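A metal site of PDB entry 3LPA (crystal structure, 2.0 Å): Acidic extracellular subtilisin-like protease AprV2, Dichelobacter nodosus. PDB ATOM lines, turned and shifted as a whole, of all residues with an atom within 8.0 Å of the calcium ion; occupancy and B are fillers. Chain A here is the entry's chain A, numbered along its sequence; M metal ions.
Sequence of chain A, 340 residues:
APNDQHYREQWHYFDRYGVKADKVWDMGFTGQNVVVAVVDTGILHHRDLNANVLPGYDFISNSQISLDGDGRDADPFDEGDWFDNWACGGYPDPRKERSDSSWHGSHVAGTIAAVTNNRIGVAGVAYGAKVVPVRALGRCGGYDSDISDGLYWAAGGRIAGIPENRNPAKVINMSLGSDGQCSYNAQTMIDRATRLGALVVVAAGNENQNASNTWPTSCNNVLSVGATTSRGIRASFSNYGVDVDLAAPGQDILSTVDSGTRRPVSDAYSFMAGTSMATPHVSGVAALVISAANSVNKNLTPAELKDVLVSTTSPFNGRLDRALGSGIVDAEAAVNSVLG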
ATOM      1  N   PRO A   2      16.906 -21.612  25.176  1.00  0.00           N
ATOM      2  CA  PRO A   2      16.062 -20.446  24.859  1.00  0.00           C
ATOM      3  C   PRO A   2      16.850 -19.313  24.195  1.00  0.00           C
ATOM      4  O   PRO A   2      17.997 -19.075  24.557  1.00  0.00           O
ATOM      5  CB  PRO A   2      15.571 -19.967  26.230  1.00  0.00           C
ATOM      6  CG  PRO A   2      15.749 -21.115  27.136  1.00  0.00           C
ATOM      7  CD  PRO A   2      16.921 -21.883  26.629  1.00  0.00           C
ATOM      8  N   ASN A   3      16.219 -18.620  23.248  1.00  0.00           N
ATOM      9  CA  ASN A   3      16.896 -17.526  22.528  1.00  0.00           C
ATOM     10  C   ASN A   3      16.855 -16.155  23.222  1.00  0.00           C
ATOM     11  O   ASN A   3      17.408 -15.187  22.700  1.00  0.00           O
ATOM     12  CB  ASN A   3      16.376 -17.421  21.076  1.00  0.00           C
ATOM     13  CG  ASN A   3      14.966 -16.823  20.973  1.00  0.00           C
ATOM     14  OD1 ASN A   3      14.479 -16.171  21.887  1.00  0.00           O
ATOM     15  ND2 ASN A   3      14.324 -17.044  19.834  1.00  0.00           N
ATOM     16  N   ASP A   4      16.211 -16.091  24.389  1.00  0.00           N
ATOM     17  CA  ASP A   4      15.941 -14.800  25.025  1.00  0.00           C
ATOM     18  C   ASP A   4      17.207 -14.041  25.445  1.00  0.00           C
ATOM     19  O   ASP A   4      18.167 -14.624  25.978  1.00  0.00           O
ATOM     20  CB  ASP A   4      14.990 -14.975  26.207  1.00  0.00           C
ATOM     21  CG  ASP A   4      13.714 -15.672  25.812  1.00  0.00           C
ATOM     22  OD1 ASP A   4      12.705 -14.976  25.598  1.00  0.00           O
ATOM     23  OD2 ASP A   4      13.716 -16.919  25.729  1.00  0.00           O
ATOM     24  N   GLN A   5      17.202 -12.726  25.198  1.00  0.00           N
ATOM     25  CA  GLN A   5      18.351 -11.848  25.404  1.00  0.00           C
ATOM     26  C   GLN A   5      19.054 -12.035  26.771  1.00  0.00           C
ATOM     27  O   GLN A   5      20.286 -12.116  26.845  1.00  0.00           O
ATOM     28  CB  GLN A   5      17.913 -10.391  25.221  1.00  0.00           C
ATOM     29  CG  GLN A   5      19.004  -9.391  24.878  1.00  0.00           C
ATOM     30  CD  GLN A   5      19.500  -9.510  23.430  1.00  0.00           C
ATOM     31  OE1 GLN A   5      18.945 -10.240  22.605  1.00  0.00           O
ATOM     32  NE2 GLN A   5      20.587  -8.796  23.128  1.00  0.00           N
ATOM     33  N   HIS A   6      18.279 -12.114  27.850  1.00  0.00           N
ATOM     34  CA  HIS A   6      18.878 -12.147  29.184  1.00  0.00           C
ATOM     35  C   HIS A   6      18.752 -13.473  29.899  1.00  0.00           C
ATOM     36  O   HIS A   6      18.999 -13.542  31.101  1.00  0.00           O
ATOM     37  CB  HIS A   6      18.349 -10.993  30.080  1.00  0.00           C
ATOM     38  CG  HIS A   6      18.405  -9.650  29.423  1.00  0.00           C
ATOM     39  ND1 HIS A   6      19.563  -8.905  29.337  1.00  0.00           N
ATOM     40  CD2 HIS A   6      17.444  -8.930  28.789  1.00  0.00           C
ATOM     41  CE1 HIS A   6      19.307  -7.789  28.697  1.00  0.00           C
ATOM     42  NE2 HIS A   6      18.026  -7.775  28.349  1.00  0.00           N
ATOM     43  N   TYR A   7      18.414 -14.531  29.145  1.00  0.00           N
ATOM     44  CA  TYR A   7      18.422 -15.903  29.702  1.00  0.00           C
ATOM     45  C   TYR A   7      19.734 -16.234  30.435  1.00  0.00           C
ATOM     46  O   TYR A   7      19.720 -16.872  31.486  1.00  0.00           O
ATOM     47  CB  TYR A   7      18.174 -16.930  28.604  1.00  0.00           C
ATOM     48  CG  TYR A   7      18.413 -18.359  29.046  1.00  0.00           C
ATOM     49  CD1 TYR A   7      17.509 -19.001  29.891  1.00  0.00           C
ATOM     50  CD2 TYR A   7      19.564 -19.048  28.628  1.00  0.00           C
ATOM     51  CE1 TYR A   7      17.720 -20.314  30.299  1.00  0.00           C
ATOM     52  CE2 TYR A   7      19.807 -20.379  29.041  1.00  0.00           C
ATOM     53  CZ  TYR A   7      18.880 -21.005  29.871  1.00  0.00           C
ATOM     54  OH  TYR A   7      19.106 -22.297  30.289  1.00  0.00           O
ATOM     55  N   GLN A  10      19.842 -15.681  34.159  1.00  0.00           N
ATOM     56  CA  GLN A  10      18.991 -16.511  35.008  1.00  0.00           C
ATOM     57  C   GLN A  10      19.692 -17.811  35.476  1.00  0.00           C
ATOM     58  O   GLN A  10      19.206 -18.917  35.231  1.00  0.00           O
ATOM     59  CB  GLN A  10      17.667 -16.795  34.278  1.00  0.00           C
ATOM     60  CG  GLN A  10      17.030 -15.502  33.783  1.00  0.00           C
ATOM     61  CD  GLN A  10      15.645 -15.697  33.220  1.00  0.00           C
ATOM     62  OE1 GLN A  10      15.468 -16.081  32.050  1.00  0.00           O
ATOM     63  NE2 GLN A  10      14.629 -15.410  34.051  1.00  0.00           N
ATOM     64  N   HIS A  46       2.696  -6.736  29.863  1.00  0.00           N
ATOM     65  CA  HIS A  46       4.144  -6.728  29.608  1.00  0.00           C
ATOM     66  C   HIS A  46       4.406  -7.527  28.353  1.00  0.00           C
ATOM     67  O   HIS A  46       3.972  -8.677  28.255  1.00  0.00           O
ATOM     68  CB  HIS A  46       4.833  -7.362  30.811  1.00  0.00           C
ATOM     69  CG  HIS A  46       6.307  -7.112  30.905  1.00  0.00           C
ATOM     70  ND1 HIS A  46       7.221  -7.676  30.035  1.00  0.00           N
ATOM     71  CD2 HIS A  46       7.033  -6.430  31.811  1.00  0.00           C
ATOM     72  CE1 HIS A  46       8.442  -7.329  30.390  1.00  0.00           C
ATOM     73  NE2 HIS A  46       8.359  -6.567  31.458  1.00  0.00           N
ATOM     74  N   ARG A  47       5.112  -6.952  27.389  1.00  0.00           N
ATOM     75  CA  ARG A  47       5.422  -7.672  26.151  1.00  0.00           C
ATOM     76  C   ARG A  47       6.006  -9.060  26.395  1.00  0.00           C
ATOM     77  O   ARG A  47       5.856  -9.942  25.551  1.00  0.00           O
ATOM     78  CB  ARG A  47       6.341  -6.836  25.238  1.00  0.00           C
ATOM     79  CG  ARG A  47       5.585  -5.892  24.331  1.00  0.00           C
ATOM     80  CD  ARG A  47       6.502  -5.177  23.336  1.00  0.00           C
ATOM     81  N   ASP A  48       6.659  -9.277  27.548  1.00  0.00           N
ATOM     82  CA  ASP A  48       7.292 -10.586  27.808  1.00  0.00           C
ATOM     83  C   ASP A  48       6.423 -11.466  28.750  1.00  0.00           C
ATOM     84  O   ASP A  48       6.905 -12.480  29.272  1.00  0.00           O
ATOM     85  CB  ASP A  48       8.739 -10.429  28.329  1.00  0.00           C
ATOM     86  CG  ASP A  48       9.697 -11.511  27.764  1.00  0.00           C
ATOM     87  OD1 ASP A  48       9.513 -11.913  26.582  1.00  0.00           O
ATOM     88  OD2 ASP A  48      10.676 -11.948  28.477  1.00  0.00           O
ATOM     89  N   LEU A  49       5.161 -11.072  28.947  1.00  0.00           N
ATOM     90  CA  LEU A  49       4.147 -11.874  29.668  1.00  0.00           C
ATOM     91  C   LEU A  49       2.862 -12.100  28.854  1.00  0.00           C
ATOM     92  O   LEU A  49       2.275 -13.195  28.904  1.00  0.00           O
ATOM     93  CB  LEU A  49       3.756 -11.221  31.033  1.00  0.00           C
ATOM     94  CG  LEU A  49       4.885 -11.026  32.041  1.00  0.00           C
ATOM     95  CD1 LEU A  49       4.359 -10.185  33.198  1.00  0.00           C
ATOM     96  CD2 LEU A  49       5.406 -12.397  32.526  1.00  0.00           C
ATOM     97  N   ALA A 114       7.267 -16.619  31.866  1.00  0.00           N
ATOM     98  CA  ALA A 114       7.627 -15.499  31.004  1.00  0.00           C
ATOM     99  C   ALA A 114       7.673 -16.075  29.596  1.00  0.00           C
ATOM    100  O   ALA A 114       8.098 -17.216  29.411  1.00  0.00           O
ATOM    101  CB  ALA A 114       8.994 -14.879  31.394  1.00  0.00           C
ATOM    102  N   VAL A 115       7.172 -15.295  28.641  1.00  0.00           N
ATOM    103  CA  VAL A 115       7.252 -15.654  27.225  1.00  0.00           C
ATOM    104  C   VAL A 115       8.712 -15.944  26.815  1.00  0.00           C
ATOM    105  O   VAL A 115       9.582 -15.086  26.935  1.00  0.00           O
ATOM    106  CB  VAL A 115       6.630 -14.567  26.303  1.00  0.00           C
ATOM    107  CG1 VAL A 115       6.547 -15.072  24.838  1.00  0.00           C
ATOM    108  CG2 VAL A 115       5.238 -14.181  26.782  1.00  0.00           C
ATOM    109  N   THR A 116       8.941 -17.156  26.318  1.00  0.00           N
ATOM    110  CA  THR A 116      10.259 -17.666  26.014  1.00  0.00           C
ATOM    111  C   THR A 116      10.416 -17.920  24.518  1.00  0.00           C
ATOM    112  O   THR A 116       9.465 -18.247  23.831  1.00  0.00           O
ATOM    113  CB  THR A 116      10.476 -18.938  26.819  1.00  0.00           C
ATOM    114  OG1 THR A 116      10.293 -18.632  28.191  1.00  0.00           O
ATOM    115  CG2 THR A 116      11.866 -19.547  26.603  1.00  0.00           C
ATOM    116  N   ASN A 117      11.651 -17.768  24.033  1.00  0.00           N
ATOM    117  CA  ASN A 117      11.969 -17.927  22.615  1.00  0.00           C
ATOM    118  C   ASN A 117      11.378 -16.845  21.712  1.00  0.00           C
ATOM    119  O   ASN A 117      11.278 -17.029  20.500  1.00  0.00           O
ATOM    120  CB  ASN A 117      11.656 -19.360  22.137  1.00  0.00           C
ATOM    121  CG  ASN A 117      12.658 -20.375  22.681  1.00  0.00           C
ATOM    122  OD1 ASN A 117      13.872 -20.151  22.668  1.00  0.00           O
ATOM    123  ND2 ASN A 117      12.159 -21.515  23.155  1.00  0.00           N
ATOM    124  N   ASN A 118      10.990 -15.721  22.307  1.00  0.00           N
ATOM    125  CA  ASN A 118      10.579 -14.525  21.574  1.00  0.00           C
ATOM    126  C   ASN A 118      11.677 -13.459  21.554  1.00  0.00           C
ATOM    127  O   ASN A 118      11.383 -12.283  21.384  1.00  0.00           O
ATOM    128  CB  ASN A 118       9.282 -13.952  22.168  1.00  0.00           C
ATOM    129  CG  ASN A 118       9.487 -13.356  23.568  1.00  0.00           C
ATOM    130  OD1 ASN A 118      10.413 -13.747  24.290  1.00  0.00           O
ATOM    131  ND2 ASN A 118       8.621 -12.419  23.949  1.00  0.00           N
ATOM    132  N   ARG A 119      12.927 -13.867  21.759  1.00  0.00           N
ATOM    133  CA  ARG A 119      14.123 -12.974  21.723  1.00  0.00           C
ATOM    134  C   ARG A 119      14.250 -11.882  22.820  1.00  0.00           C
ATOM    135  O   ARG A 119      15.356 -11.646  23.349  1.00  0.00           O
ATOM    136  CB  ARG A 119      14.344 -12.371  20.314  1.00  0.00           C
ATOM    137  N   ILE A 120      13.153 -11.213  23.156  1.00  0.00           N
ATOM    138  CA  ILE A 120      13.223 -10.134  24.116  1.00  0.00           C
ATOM    139  C   ILE A 120      13.308 -10.703  25.537  1.00  0.00           C
ATOM    140  O   ILE A 120      12.824 -11.815  25.793  1.00  0.00           O
ATOM    141  CB  ILE A 120      12.048  -9.088  24.000  1.00  0.00           C
ATOM    142  CG1 ILE A 120      10.675  -9.746  24.151  1.00  0.00           C
ATOM    143  CG2 ILE A 120      12.145  -8.226  22.690  1.00  0.00           C
ATOM    144  CD1 ILE A 120       9.589  -8.791  24.627  1.00  0.00           C
ATOM    145  N   GLY A 121      14.003  -9.999  26.408  1.00  0.00           N
ATOM    146  CA  GLY A 121      13.840 -10.211  27.849  1.00  0.00           C
ATOM    147  C   GLY A 121      14.345 -11.560  28.353  1.00  0.00           C
ATOM    148  O   GLY A 121      15.500 -11.930  28.100  1.00  0.00           O
ATOM    149  N   VAL A 122      13.469 -12.273  29.064  1.00  0.00           N
ATOM    150  CA  VAL A 122      13.846 -13.453  29.859  1.00  0.00           C
ATOM    151  C   VAL A 122      13.056 -14.712  29.467  1.00  0.00           C
ATOM    152  O   VAL A 122      12.238 -14.688  28.538  1.00  0.00           O
ATOM    153  CB  VAL A 122      13.638 -13.187  31.393  1.00  0.00           C
ATOM    154  CG1 VAL A 122      14.613 -12.143  31.890  1.00  0.00           C
ATOM    155  CG2 VAL A 122      12.188 -12.782  31.669  1.00  0.00           C
ATOM    156  N   ALA A 123      13.322 -15.803  30.178  1.00  0.00           N
ATOM    157  CA  ALA A 123      12.592 -17.062  30.026  1.00  0.00           C
ATOM    158  C   ALA A 123      11.824 -17.399  31.307  1.00  0.00           C
ATOM    159  O   ALA A 123      12.086 -16.835  32.387  1.00  0.00           O
ATOM    160  CB  ALA A 123      13.558 -18.182  29.702  1.00  0.00           C
ATOM    161  N   GLY A 124      10.877 -18.330  31.202  1.00  0.00           N
ATOM    162  CA  GLY A 124      10.175 -18.861  32.364  1.00  0.00           C
ATOM    163  C   GLY A 124      10.487 -20.332  32.600  1.00  0.00           C
ATOM    164  O   GLY A 124      10.881 -21.049  31.654  1.00  0.00           O
ATOM    165  N   THR A 256      10.368 -10.334  35.128  1.00  0.00           N
ATOM    166  CA  THR A 256       9.685  -9.253  34.453  1.00  0.00           C
ATOM    167  C   THR A 256       8.978  -8.307  35.428  1.00  0.00           C
ATOM    168  O   THR A 256       8.222  -8.760  36.298  1.00  0.00           O
ATOM    169  CB  THR A 256       8.615  -9.891  33.532  1.00  0.00           C
ATOM    170  OG1 THR A 256       7.880 -10.860  34.285  1.00  0.00           O
ATOM    171  CG2 THR A 256       9.282 -10.626  32.364  1.00  0.00           C
ATOM    172  N   TYR A 269      12.899  -5.310  33.571  1.00  0.00           N
ATOM    173  CA  TYR A 269      13.363  -6.559  34.170  1.00  0.00           C
ATOM    174  C   TYR A 269      14.155  -6.214  35.429  1.00  0.00           C
ATOM    175  O   TYR A 269      14.846  -5.189  35.471  1.00  0.00           O
ATOM    176  CB  TYR A 269      14.231  -7.348  33.170  1.00  0.00           C
ATOM    177  CG  TYR A 269      13.482  -7.584  31.878  1.00  0.00           C
ATOM    178  CD1 TYR A 269      12.677  -8.728  31.728  1.00  0.00           C
ATOM    179  CD2 TYR A 269      13.495  -6.621  30.868  1.00  0.00           C
ATOM    180  CE1 TYR A 269      11.942  -8.933  30.528  1.00  0.00           C
ATOM    181  CE2 TYR A 269      12.757  -6.807  29.691  1.00  0.00           C
ATOM    182  CZ  TYR A 269      11.980  -7.962  29.540  1.00  0.00           C
ATOM    183  OH  TYR A 269      11.259  -8.133  28.365  1.00  0.00           O
HETATM  184 CA    CA M   1      11.306 -13.578  26.513  1.00  0.00          CA
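The side-chain carboxylate of Asp 4 lies within hydrogen-bond range of the backbone NH of Asn 117, at 2.8 Å.
A ring nitrogen (ND1) of His 46 lies close to the backbone NH of Asp 48 (3.0 Å).
Six residues have an atom within 4 Å of the calcium ion: Asp 4, Asp 48, Val 115, Asn 118, Ile 120 and Val 122.
The nearest printed residue that does not touch the calcium ion is Gly 121 (4.1 Å).
The side-chain carboxylate (OD1) of Asp 4 binds the calcium ion (2.2 Å).
The calcium ion is bound by the backbone carbonyl oxygen (O) of Val 115 (2.3 Å).
OD1 of Asn 118 is bound to the calcium ion (2.4 Å).
The backbone carbonyl oxygen (O) of Ile 120 is bound to the calcium ion (2.4 Å).
The side-chain carboxylate (OD1) of Asp 48 is bound to the calcium ion, 2.4 Å away.
The calcium ion is bound by O of Val 122, 2.5 Å away.
The side-chain carboxylate (OD2) of Asp 48 is bound to the calcium ion (2.6 Å).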
